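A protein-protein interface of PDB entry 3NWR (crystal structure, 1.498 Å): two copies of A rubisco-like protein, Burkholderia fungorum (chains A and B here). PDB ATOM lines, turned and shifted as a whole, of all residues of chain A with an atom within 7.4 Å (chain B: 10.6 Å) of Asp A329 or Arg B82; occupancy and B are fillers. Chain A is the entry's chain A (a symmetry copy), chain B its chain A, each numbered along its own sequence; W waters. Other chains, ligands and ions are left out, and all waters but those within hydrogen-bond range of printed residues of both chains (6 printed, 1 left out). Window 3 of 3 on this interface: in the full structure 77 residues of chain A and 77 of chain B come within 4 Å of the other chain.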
ATOM      1  N   VAL A 318      25.694  22.443  -3.206  1.00  0.00           N
ATOM      2  CA  VAL A 318      24.499  21.646  -2.944  1.00  0.00           C
ATOM      3  C   VAL A 318      23.934  21.854  -1.541  1.00  0.00           C
ATOM      4  O   VAL A 318      22.973  21.185  -1.152  1.00  0.00           O
ATOM      5  CB  VAL A 318      24.767  20.140  -3.158  1.00  0.00           C
ATOM      6  CG1 VAL A 318      25.220  19.885  -4.585  1.00  0.00           C
ATOM      7  CG2 VAL A 318      25.799  19.604  -2.165  1.00  0.00           C
ATOM      8  N   GLY A 320      23.823  21.435   2.450  1.00  0.00           N
ATOM      9  CA  GLY A 320      24.359  20.381   3.302  1.00  0.00           C
ATOM     10  C   GLY A 320      23.362  19.575   4.094  1.00  0.00           C
ATOM     11  O   GLY A 320      22.290  20.069   4.438  1.00  0.00           O
ATOM     12  N   LEU A 321      23.730  18.334   4.396  1.00  0.00           N
ATOM     13  CA  LEU A 321      22.910  17.479   5.244  1.00  0.00           C
ATOM     14  C   LEU A 321      22.909  18.014   6.671  1.00  0.00           C
ATOM     15  O   LEU A 321      23.946  18.431   7.187  1.00  0.00           O
ATOM     16  CB  LEU A 321      23.441  16.046   5.200  1.00  0.00           C
ATOM     17  CG  LEU A 321      23.410  15.446   3.792  1.00  0.00           C
ATOM     18  CD1 LEU A 321      24.006  14.055   3.806  1.00  0.00           C
ATOM     19  CD2 LEU A 321      21.988  15.442   3.215  1.00  0.00           C
ATOM     20  N   ALA A 322      21.732  18.015   7.292  1.00  0.00           N
ATOM     21  CA  ALA A 322      21.549  18.586   8.622  1.00  0.00           C
ATOM     22  C   ALA A 322      22.019  20.035   8.661  1.00  0.00           C
ATOM     23  O   ALA A 322      22.541  20.502   9.668  1.00  0.00           O
ATOM     24  CB  ALA A 322      22.295  17.753   9.675  1.00  0.00           C
ATOM     25  N   GLY A 323      21.825  20.752   7.561  1.00  0.00           N
ATOM     26  CA  GLY A 323      22.342  22.106   7.468  1.00  0.00           C
ATOM     27  C   GLY A 323      21.503  23.129   8.204  1.00  0.00           C
ATOM     28  O   GLY A 323      20.478  22.792   8.804  1.00  0.00           O
ATOM     29  N   LYS A 324      21.940  24.384   8.150  1.00  0.00           N
ATOM     30  CA  LYS A 324      21.227  25.476   8.806  1.00  0.00           C
ATOM     31  C   LYS A 324      20.316  26.234   7.835  1.00  0.00           C
ATOM     32  O   LYS A 324      19.547  27.093   8.250  1.00  0.00           O
ATOM     33  CB  LYS A 324      22.220  26.431   9.473  1.00  0.00           C
ATOM     34  CG  LYS A 324      23.086  25.745  10.526  1.00  0.00           C
ATOM     35  CD  LYS A 324      24.063  26.704  11.193  1.00  0.00           C
ATOM     36  CE  LYS A 324      24.918  25.964  12.212  1.00  0.00           C
ATOM     37  NZ  LYS A 324      25.751  26.892  13.029  1.00  0.00           N
ATOM     38  N   PHE A 325      20.401  25.899   6.549  1.00  0.00           N
ATOM     39  CA  PHE A 325      19.530  26.486   5.534  1.00  0.00           C
ATOM     40  C   PHE A 325      18.164  25.782   5.502  1.00  0.00           C
ATOM     41  O   PHE A 325      17.925  24.812   6.236  1.00  0.00           O
ATOM     42  CB  PHE A 325      20.182  26.366   4.145  1.00  0.00           C
ATOM     43  CG  PHE A 325      21.363  27.287   3.911  1.00  0.00           C
ATOM     44  CD1 PHE A 325      21.271  28.647   4.137  1.00  0.00           C
ATOM     45  CD2 PHE A 325      22.550  26.780   3.408  1.00  0.00           C
ATOM     46  CE1 PHE A 325      22.352  29.496   3.889  1.00  0.00           C
ATOM     47  CE2 PHE A 325      23.634  27.616   3.158  1.00  0.00           C
ATOM     48  CZ  PHE A 325      23.529  28.979   3.401  1.00  0.00           C
ATOM     49  N   ALA A 326      17.280  26.243   4.622  1.00  0.00           N
ATOM     50  CA  ALA A 326      15.924  25.699   4.515  1.00  0.00           C
ATOM     51  C   ALA A 326      15.836  24.368   3.767  1.00  0.00           C
ATOM     52  O   ALA A 326      14.857  23.639   3.909  1.00  0.00           O
ATOM     53  CB  ALA A 326      15.005  26.720   3.856  1.00  0.00           C
ATOM     54  N   GLN A 327      16.840  24.054   2.958  1.00  0.00           N
ATOM     55  CA  GLN A 327      16.760  22.878   2.092  1.00  0.00           C
ATOM     56  C   GLN A 327      16.701  21.553   2.853  1.00  0.00           C
ATOM     57  O   GLN A 327      17.378  21.380   3.864  1.00  0.00           O
ATOM     58  CB  GLN A 327      17.933  22.842   1.113  1.00  0.00           C
ATOM     59  CG  GLN A 327      17.806  23.834  -0.036  1.00  0.00           C
ATOM     60  CD  GLN A 327      18.071  25.262   0.388  1.00  0.00           C
ATOM     61  OE1 GLN A 327      18.861  25.520   1.289  1.00  0.00           O
ATOM     62  NE2 GLN A 327      17.405  26.206  -0.269  1.00  0.00           N
ATOM     63  N   SER A 328      15.899  20.623   2.339  1.00  0.00           N
ATOM     64  CA  SER A 328      15.778  19.288   2.933  1.00  0.00           C
ATOM     65  C   SER A 328      16.982  18.420   2.608  1.00  0.00           C
ATOM     66  O   SER A 328      17.682  18.647   1.612  1.00  0.00           O
ATOM     67  CB  SER A 328      14.523  18.583   2.412  1.00  0.00           C
ATOM     68  OG  SER A 328      14.654  18.295   1.028  1.00  0.00           O
ATOM     69  N   ASP A 329      17.218  17.408   3.440  1.00  0.00           N
ATOM     70  CA  ASP A 329      18.287  16.463   3.162  1.00  0.00           C
ATOM     71  C   ASP A 329      18.053  15.787   1.814  1.00  0.00           C
ATOM     72  O   ASP A 329      19.002  15.555   1.062  1.00  0.00           O
ATOM     73  CB  ASP A 329      18.371  15.390   4.256  1.00  0.00           C
ATOM     74  CG  ASP A 329      19.037  15.885   5.536  1.00  0.00           C
ATOM     75  OD1 ASP A 329      19.527  17.029   5.585  1.00  0.00           O
ATOM     76  OD2 ASP A 329      19.083  15.101   6.510  1.00  0.00           O
ATOM     77  N   ALA A 330      16.800  15.453   1.508  1.00  0.00           N
ATOM     78  CA  ALA A 330      16.493  14.807   0.234  1.00  0.00           C
ATOM     79  C   ALA A 330      16.960  15.649  -0.953  1.00  0.00           C
ATOM     80  O   ALA A 330      17.544  15.118  -1.894  1.00  0.00           O
ATOM     81  CB  ALA A 330      14.989  14.486   0.113  1.00  0.00           C
ATOM     82  N   GLU A 331      16.689  16.953  -0.907  1.00  0.00           N
ATOM     83  CA  GLU A 331      17.145  17.846  -1.970  1.00  0.00           C
ATOM     84  C   GLU A 331      18.666  17.886  -2.055  1.00  0.00           C
ATOM     85  O   GLU A 331      19.235  17.878  -3.144  1.00  0.00           O
ATOM     86  CB  GLU A 331      16.588  19.272  -1.813  1.00  0.00           C
ATOM     87  CG  GLU A 331      17.171  20.214  -2.882  1.00  0.00           C
ATOM     88  CD  GLU A 331      16.501  21.579  -2.976  1.00  0.00           C
ATOM     89  OE1 GLU A 331      15.447  21.786  -2.347  1.00  0.00           O
ATOM     90  OE2 GLU A 331      17.039  22.448  -3.700  1.00  0.00           O
ATOM     91  N   VAL A 332      19.332  17.953  -0.914  1.00  0.00           N
ATOM     92  CA  VAL A 332      20.794  17.973  -0.921  1.00  0.00           C
ATOM     93  C   VAL A 332      21.364  16.686  -1.535  1.00  0.00           C
ATOM     94  O   VAL A 332      22.261  16.731  -2.366  1.00  0.00           O
ATOM     95  CB  VAL A 332      21.369  18.146   0.493  1.00  0.00           C
ATOM     96  CG1 VAL A 332      22.891  18.005   0.451  1.00  0.00           C
ATOM     97  CG2 VAL A 332      20.930  19.487   1.095  1.00  0.00           C
ATOM     98  N   ILE A 333      20.827  15.536  -1.130  1.00  0.00           N
ATOM     99  CA  ILE A 333      21.286  14.259  -1.652  1.00  0.00           C
ATOM    100  C   ILE A 333      21.104  14.174  -3.167  1.00  0.00           C
ATOM    101  O   ILE A 333      22.037  13.834  -3.891  1.00  0.00           O
ATOM    102  CB  ILE A 333      20.556  13.089  -0.972  1.00  0.00           C
ATOM    103  CG1 ILE A 333      20.940  13.038   0.508  1.00  0.00           C
ATOM    104  CG2 ILE A 333      20.910  11.773  -1.653  1.00  0.00           C
ATOM    105  CD1 ILE A 333      20.080  12.099   1.326  1.00  0.00           C
ATOM    106  N   GLU A 334      19.908  14.510  -3.644  1.00  0.00           N
ATOM    107  CA  GLU A 334      19.630  14.432  -5.072  1.00  0.00           C
ATOM    108  C   GLU A 334      20.527  15.399  -5.852  1.00  0.00           C
ATOM    109  O   GLU A 334      21.001  15.079  -6.948  1.00  0.00           O
ATOM    110  CB  GLU A 334      18.153  14.729  -5.353  1.00  0.00           C
ATOM    111  CG  GLU A 334      17.793  14.680  -6.834  1.00  0.00           C
ATOM    112  CD  GLU A 334      16.311  14.895  -7.090  1.00  0.00           C
ATOM    113  OE1 GLU A 334      15.520  14.785  -6.128  1.00  0.00           O
ATOM    114  OE2 GLU A 334      15.938  15.170  -8.253  1.00  0.00           O
ATOM    115  N   SER A 335      20.764  16.574  -5.276  1.00  0.00           N
ATOM    116  CA  SER A 335      21.568  17.595  -5.953  1.00  0.00           C
ATOM    117  C   SER A 335      23.026  17.144  -6.065  1.00  0.00           C
ATOM    118  O   SER A 335      23.664  17.308  -7.111  1.00  0.00           O
ATOM    119  CB  SER A 335      21.448  18.935  -5.221  1.00  0.00           C
ATOM    120  OG  SER A 335      20.102  19.409  -5.257  1.00  0.00           O
ATOM    121  N   ALA A 366      26.654  10.827   6.813  1.00  0.00           N
ATOM    122  CA  ALA A 366      25.513  11.048   5.931  1.00  0.00           C
ATOM    123  C   ALA A 366      25.986  11.553   4.571  1.00  0.00           C
ATOM    124  O   ALA A 366      25.444  11.184   3.524  1.00  0.00           O
ATOM    125  CB  ALA A 366      24.548  12.032   6.553  1.00  0.00           C
ATOM    126  N   ALA A 370      25.522   9.724   1.019  1.00  0.00           N
ATOM    127  CA  ALA A 370      24.845  10.421  -0.081  1.00  0.00           C
ATOM    128  C   ALA A 370      25.623  10.326  -1.395  1.00  0.00           C
ATOM    129  O   ALA A 370      25.051  10.013  -2.441  1.00  0.00           O
ATOM    130  CB  ALA A 370      24.593  11.888   0.276  1.00  0.00           C
ATOM    131  N   PRO B  24       8.416  31.962  12.077  1.00  0.00           N
ATOM    132  CA  PRO B  24       7.718  31.665  13.331  1.00  0.00           C
ATOM    133  C   PRO B  24       8.539  32.168  14.512  1.00  0.00           C
ATOM    134  O   PRO B  24       8.062  32.148  15.652  1.00  0.00           O
ATOM    135  CB  PRO B  24       7.667  30.143  13.336  1.00  0.00           C
ATOM    136  CG  PRO B  24       8.915  29.731  12.627  1.00  0.00           C
ATOM    137  CD  PRO B  24       9.153  30.793  11.564  1.00  0.00           C
ATOM    138  N   PRO B  76       8.080  25.774   2.459  1.00  0.00           N
ATOM    139  CA  PRO B  76       8.664  24.682   3.245  1.00  0.00           C
ATOM    140  C   PRO B  76      10.001  25.097   3.842  1.00  0.00           C
ATOM    141  O   PRO B  76      10.701  25.954   3.293  1.00  0.00           O
ATOM    142  CB  PRO B  76       8.903  23.581   2.204  1.00  0.00           C
ATOM    143  CG  PRO B  76       8.015  23.918   1.059  1.00  0.00           C
ATOM    144  CD  PRO B  76       7.889  25.410   1.045  1.00  0.00           C
ATOM    145  N   ASN B  77      10.360  24.483   4.960  1.00  0.00           N
ATOM    146  CA  ASN B  77      11.631  24.770   5.590  1.00  0.00           C
ATOM    147  C   ASN B  77      12.057  23.595   6.454  1.00  0.00           C
ATOM    148  O   ASN B  77      11.434  23.328   7.478  1.00  0.00           O
ATOM    149  CB  ASN B  77      11.526  26.056   6.420  1.00  0.00           C
ATOM    150  CG  ASN B  77      12.834  26.427   7.077  1.00  0.00           C
ATOM    151  OD1 ASN B  77      13.565  25.561   7.553  1.00  0.00           O
ATOM    152  ND2 ASN B  77      13.150  27.717   7.092  1.00  0.00           N
ATOM    153  N   ALA B  78      13.107  22.896   6.029  1.00  0.00           N
ATOM    154  CA  ALA B  78      13.536  21.666   6.696  1.00  0.00           C
ATOM    155  C   ALA B  78      14.141  21.905   8.077  1.00  0.00           C
ATOM    156  O   ALA B  78      13.982  21.081   8.979  1.00  0.00           O
ATOM    157  CB  ALA B  78      14.515  20.894   5.814  1.00  0.00           C
ATOM    158  N   TRP B  79      14.839  23.022   8.244  1.00  0.00           N
ATOM    159  CA  TRP B  79      15.450  23.343   9.525  1.00  0.00           C
ATOM    160  C   TRP B  79      14.371  23.602  10.572  1.00  0.00           C
ATOM    161  O   TRP B  79      14.444  23.089  11.688  1.00  0.00           O
ATOM    162  CB  TRP B  79      16.393  24.547   9.398  1.00  0.00           C
ATOM    163  CG  TRP B  79      17.201  24.822  10.635  1.00  0.00           C
ATOM    164  CD1 TRP B  79      18.356  24.199  11.019  1.00  0.00           C
ATOM    165  CD2 TRP B  79      16.915  25.794  11.647  1.00  0.00           C
ATOM    166  NE1 TRP B  79      18.804  24.724  12.210  1.00  0.00           N
ATOM    167  CE2 TRP B  79      17.937  25.704  12.615  1.00  0.00           C
ATOM    168  CE3 TRP B  79      15.893  26.735  11.826  1.00  0.00           C
ATOM    169  CZ2 TRP B  79      17.966  26.519  13.748  1.00  0.00           C
ATOM    170  CZ3 TRP B  79      15.923  27.545  12.954  1.00  0.00           C
ATOM    171  CH2 TRP B  79      16.953  27.430  13.901  1.00  0.00           C
ATOM    172  N   LEU B  80      13.357  24.375  10.203  1.00  0.00           N
ATOM    173  CA  LEU B  80      12.288  24.685  11.143  1.00  0.00           C
ATOM    174  C   LEU B  80      11.473  23.447  11.502  1.00  0.00           C
ATOM    175  O   LEU B  80      11.070  23.278  12.651  1.00  0.00           O
ATOM    176  CB  LEU B  80      11.383  25.795  10.603  1.00  0.00           C
ATOM    177  CG  LEU B  80      12.000  27.193  10.647  1.00  0.00           C
ATOM    178  CD1 LEU B  80      11.125  28.194   9.905  1.00  0.00           C
ATOM    179  CD2 LEU B  80      12.218  27.637  12.091  1.00  0.00           C
ATOM    180  N   GLU B  81      11.230  22.570  10.536  1.00  0.00           N
ATOM    181  CA  GLU B  81      10.429  21.397  10.857  1.00  0.00           C
ATOM    182  C   GLU B  81      11.226  20.328  11.600  1.00  0.00           C
ATOM    183  O   GLU B  81      10.662  19.584  12.399  1.00  0.00           O
ATOM    184  CB  GLU B  81       9.697  20.830   9.640  1.00  0.00           C
ATOM    185  CG  GLU B  81      10.535  20.604   8.417  1.00  0.00           C
ATOM    186  CD  GLU B  81       9.670  20.410   7.188  1.00  0.00           C
ATOM    187  OE1 GLU B  81       8.427  20.374   7.337  1.00  0.00           O
ATOM    188  OE2 GLU B  81      10.223  20.307   6.074  1.00  0.00           O
ATOM    189  N   ARG B  82      12.532  20.270  11.356  1.00  0.00           N
ATOM    190  CA  ARG B  82      13.405  19.393  12.134  1.00  0.00           C
ATOM    191  C   ARG B  82      13.248  19.691  13.620  1.00  0.00           C
ATOM    192  O   ARG B  82      13.578  18.863  14.470  1.00  0.00           O
ATOM    193  CB  ARG B  82      14.876  19.567  11.736  1.00  0.00           C
ATOM    194  CG  ARG B  82      15.389  18.529  10.752  1.00  0.00           C
ATOM    195  CD  ARG B  82      16.913  18.428  10.770  1.00  0.00           C
ATOM    196  NE  ARG B  82      17.569  19.596  10.186  1.00  0.00           N
ATOM    197  CZ  ARG B  82      17.724  19.788   8.879  1.00  0.00           C
ATOM    198  NH1 ARG B  82      17.260  18.894   8.013  1.00  0.00           N
ATOM    199  NH2 ARG B  82      18.339  20.875   8.434  1.00  0.00           N
ATOM    200  N   GLN B  83      12.738  20.876  13.928  1.00  0.00           N
ATOM    201  CA  GLN B  83      12.630  21.312  15.314  1.00  0.00           C
ATOM    202  C   GLN B  83      11.201  21.555  15.764  1.00  0.00           C
ATOM    203  O   GLN B  83      10.969  22.054  16.866  1.00  0.00           O
ATOM    204  CB  GLN B  83      13.457  22.572  15.519  1.00  0.00           C
ATOM    205  CG  GLN B  83      14.932  22.323  15.374  1.00  0.00           C
ATOM    206  CD  GLN B  83      15.702  23.604  15.244  1.00  0.00           C
ATOM    207  OE1 GLN B  83      15.173  24.608  14.768  1.00  0.00           O
ATOM    208  NE2 GLN B  83      16.962  23.582  15.662  1.00  0.00           N
ATOM    209  N   GLY B  84      10.246  21.195  14.914  1.00  0.00           N
ATOM    210  CA  GLY B  84       8.842  21.357  15.243  1.00  0.00           C
ATOM    211  C   GLY B  84       8.515  22.725  15.809  1.00  0.00           C
ATOM    212  O   GLY B  84       7.705  22.847  16.728  1.00  0.00           O
ATOM    213  N   THR B  85       9.147  23.762  15.268  1.00  0.00           N
ATOM    214  CA  THR B  85       8.837  25.124  15.682  1.00  0.00           C
ATOM    215  C   THR B  85       7.361  25.400  15.407  1.00  0.00           C
ATOM    216  O   THR B  85       6.890  25.207  14.285  1.00  0.00           O
ATOM    217  CB  THR B  85       9.714  26.156  14.940  1.00  0.00           C
ATOM    218  OG1 THR B  85      11.082  25.729  14.968  1.00  0.00           O
ATOM    219  CG2 THR B  85       9.604  27.521  15.595  1.00  0.00           C
ATOM    220  N   PRO B  86       6.618  25.833  16.435  1.00  0.00           N
ATOM    221  CA  PRO B  86       5.181  26.066  16.274  1.00  0.00           C
ATOM    222  C   PRO B  86       4.889  27.391  15.578  1.00  0.00           C
ATOM    223  O   PRO B  86       5.714  28.307  15.619  1.00  0.00           O
ATOM    224  CB  PRO B  86       4.682  26.122  17.716  1.00  0.00           C
ATOM    225  CG  PRO B  86       5.835  26.689  18.472  1.00  0.00           C
ATOM    226  CD  PRO B  86       7.085  26.179  17.790  1.00  0.00           C
ATOM    227  N   ASP B 120      17.555  31.608   1.506  1.00  0.00           N
ATOM    228  CA  ASP B 120      17.755  30.240   1.997  1.00  0.00           C
ATOM    229  C   ASP B 120      17.774  30.109   3.514  1.00  0.00           C
ATOM    230  O   ASP B 120      17.939  29.003   4.031  1.00  0.00           O
ATOM    231  CB  ASP B 120      19.080  29.682   1.466  1.00  0.00           C
ATOM    232  CG  ASP B 120      19.106  29.568  -0.044  1.00  0.00           C
ATOM    233  OD1 ASP B 120      18.234  28.872  -0.602  1.00  0.00           O
ATOM    234  OD2 ASP B 120      20.026  30.153  -0.655  1.00  0.00           O
ATOM    235  N   LEU B 121      17.658  31.225   4.224  1.00  0.00           N
ATOM    236  CA  LEU B 121      17.839  31.201   5.678  1.00  0.00           C
ATOM    237  C   LEU B 121      16.918  30.199   6.353  1.00  0.00           C
ATOM    238  O   LEU B 121      15.727  30.143   6.063  1.00  0.00           O
ATOM    239  CB  LEU B 121      17.616  32.594   6.278  1.00  0.00           C
ATOM    240  CG  LEU B 121      18.612  33.687   5.881  1.00  0.00           C
ATOM    241  CD1 LEU B 121      18.184  35.001   6.484  1.00  0.00           C
ATOM    242  CD2 LEU B 121      20.014  33.345   6.336  1.00  0.00           C
ATOM    243  N   GLY B 122      17.483  29.418   7.270  1.00  0.00           N
ATOM    244  CA  GLY B 122      16.698  28.445   8.007  1.00  0.00           C
ATOM    245  C   GLY B 122      15.655  29.103   8.887  1.00  0.00           C
ATOM    246  O   GLY B 122      14.666  28.473   9.264  1.00  0.00           O
ATOM    247  N   GLU B 123      15.866  30.380   9.199  1.00  0.00           N
ATOM    248  CA  GLU B 123      14.951  31.117  10.070  1.00  0.00           C
ATOM    249  C   GLU B 123      13.631  31.498   9.407  1.00  0.00           C
ATOM    250  O   GLU B 123      12.652  31.786  10.094  1.00  0.00           O
ATOM    251  CB  GLU B 123      15.617  32.391  10.602  1.00  0.00           C
ATOM    252  CG  GLU B 123      16.702  32.158  11.624  1.00  0.00           C
ATOM    253  CD  GLU B 123      18.062  31.928  11.000  1.00  0.00           C
ATOM    254  OE1 GLU B 123      18.154  31.831   9.755  1.00  0.00           O
ATOM    255  OE2 GLU B 123      19.050  31.833  11.762  1.00  0.00           O
ATOM    256  N   THR B 125      10.289  31.467   6.545  1.00  0.00           N
ATOM    257  CA  THR B 125       9.343  30.766   5.686  1.00  0.00           C
ATOM    258  C   THR B 125       8.827  31.706   4.596  1.00  0.00           C
ATOM    259  O   THR B 125       7.875  31.393   3.882  1.00  0.00           O
ATOM    260  CB  THR B 125       8.170  30.173   6.501  1.00  0.00           C
ATOM    261  OG1 THR B 125       7.551  31.201   7.294  1.00  0.00           O
ATOM    262  CG2 THR B 125       8.688  29.067   7.408  1.00  0.00           C
HETATM  263  O   HOH W   1      18.732  19.537   5.504  1.00  0.00           O
HETATM  264  O   HOH W   2      18.805  27.127  -2.529  1.00  0.00           O
HETATM  265  O   HOH W   3      18.968  16.436   9.054  1.00  0.00           O
HETATM  266  O   HOH W   4      12.457  22.562   2.620  1.00  0.00           O
HETATM  267  O   HOH W   5      15.460  17.100   5.823  1.00  0.00           O
HETATM  268  O   HOH W   6      20.067  30.444   8.361  1.00  0.00           O
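Of the 19 printed residues of chain A, 8 touch a printed residue of chain B.
Hydrophobic or aromatic side chains of chain A that line the printed part of chain B: Phe A325 and Ala A326.
Of the 17 printed residues of chain B, 6 touch a printed residue of chain A.
Printed residues of chain B that touch a printed residue of chain A: Asn B77, Ala B78, Trp B79, Arg B82, Asp B120 and Gly B122.
Hydrophobic or aromatic side chains of chain B within 4 Å of the printed part of chain A: Ala B78 and Trp B79.
Among the printed residues, 15 pairs touch across the chains.
No position is printed for both chains.
The backbone carbonyl oxygen (O) of Ala A326 is in hydrogen-bond range of the backbone NH (N) of Ala B78, 2.8 Å away.
The backbone carbonyl oxygen (O) of Lys A324 lies close to the backbone NH (N) of Gly B122.
O of Asp B120 sits at hydrogen-bond distance from N of Ala A326 (2.9 Å).
The guanidinium group of Arg B82 is in salt-bridge range of the side-chain carboxylate of Asp A329, at 3.8 Å.
The side-chain amide nitrogen of Gln A327 lies within hydrogen-bond range of the side-chain carboxylate of Asp B120 (2.8 Å).
The guanidinium group (NH2) of Arg B82 is in hydrogen-bond range of the backbone carbonyl oxygen (O) of Gly A323, at 2.9 Å.
No residue of chain B comes within 4 Å of Leu A321.
Printed residues of chain B within 4 Å of Ala A322: Arg B82.
Of chain B, only Trp B79 and Arg B82 come within 4 Å of Gly A323.
Of the printed residues of chain B, Lys A324 touches Trp B79 (3.8 Å) and Gly B122 (3.2 Å).
Ser A328 touches just one residue of chain B: Ala B78 (3.5 Å).
Asp A329 touches just one residue of chain B: Arg B82.
No residue of chain B comes within 4 Å of Ala A330.
No residue of chain B comes within 4 Å of Val A332.
No residue of chain B comes within 4 Å of Ile A333.
Of chain A, only Ala A322, Gly A323 and Asp A329 come within 4 Å of Arg B82.
Gln B83 touches none of the printed residues of chain A.
Of the printed residues of chain A, Gly B122 touches Lys A324 and Phe A325.
The nearest residue of chain A that does not touch Arg B82 is Phe A325 (4.5 Å).
The nearest printed residue of chain A that does not touch Asp B120 is Lys A324 (4.9 Å).
Water W1 lies within hydrogen-bond range of OD1 of Asp A329, O of Gln A327 and NH1 of Arg B82.
Water W2 lies within hydrogen-bond range of OD1 of Asp B120 and NE2 of Gln A327.
Water W6 lies within hydrogen-bond range of OE1 of Glu B123 (2.7 Å), N of Gly B122 (3.0 Å) and O of Lys A324 (3.4 Å).
Water W3 bridges the side-chain carboxylate (OD2) of Asp A329 (2.9 Å) and the guanidinium group (NH1) of Arg B82 (3.2 Å).
Water W4 bridges O of Ala A326 (2.9 Å) and N of Ala B78 (3.5 Å).
Water W5 lies within hydrogen-bond range of N of Asp A329 (3.0 Å) and NH1 of Arg B82 (3.4 Å).
Among the printed residues, pairs that only touch across the chains: Phe A325 with Asp B120, Gly A323 with Trp B79, Gln A327 with Ala B78, Phe A325 with Trp B79, Ser A328 with Ala B78, Ala A322 with Arg B82, Ala A326 with Asn B77, Lys A324 with Trp B79 and Phe A325 with Gly B122.
The side-chain amide oxygen (OD1) of Asn B77 lies within hydrogen-bond range of the backbone NH (N) of Trp B79, 2.9 Å away.
The side-chain amide nitrogen (ND2) of Asn B77 sits at hydrogen-bond distance from the backbone carbonyl oxygen (O) of Gly B122 (2.8 Å).
N of Ala A322 lies within hydrogen-bond range of OD1 of Asp A329.
The side-chain amide oxygen of Asn B77 is in hydrogen-bond range of the backbone NH of Leu B80, 2.9 Å away.
OG of Ser A328 is in hydrogen-bond range of N of Glu A331 (3.1 Å).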
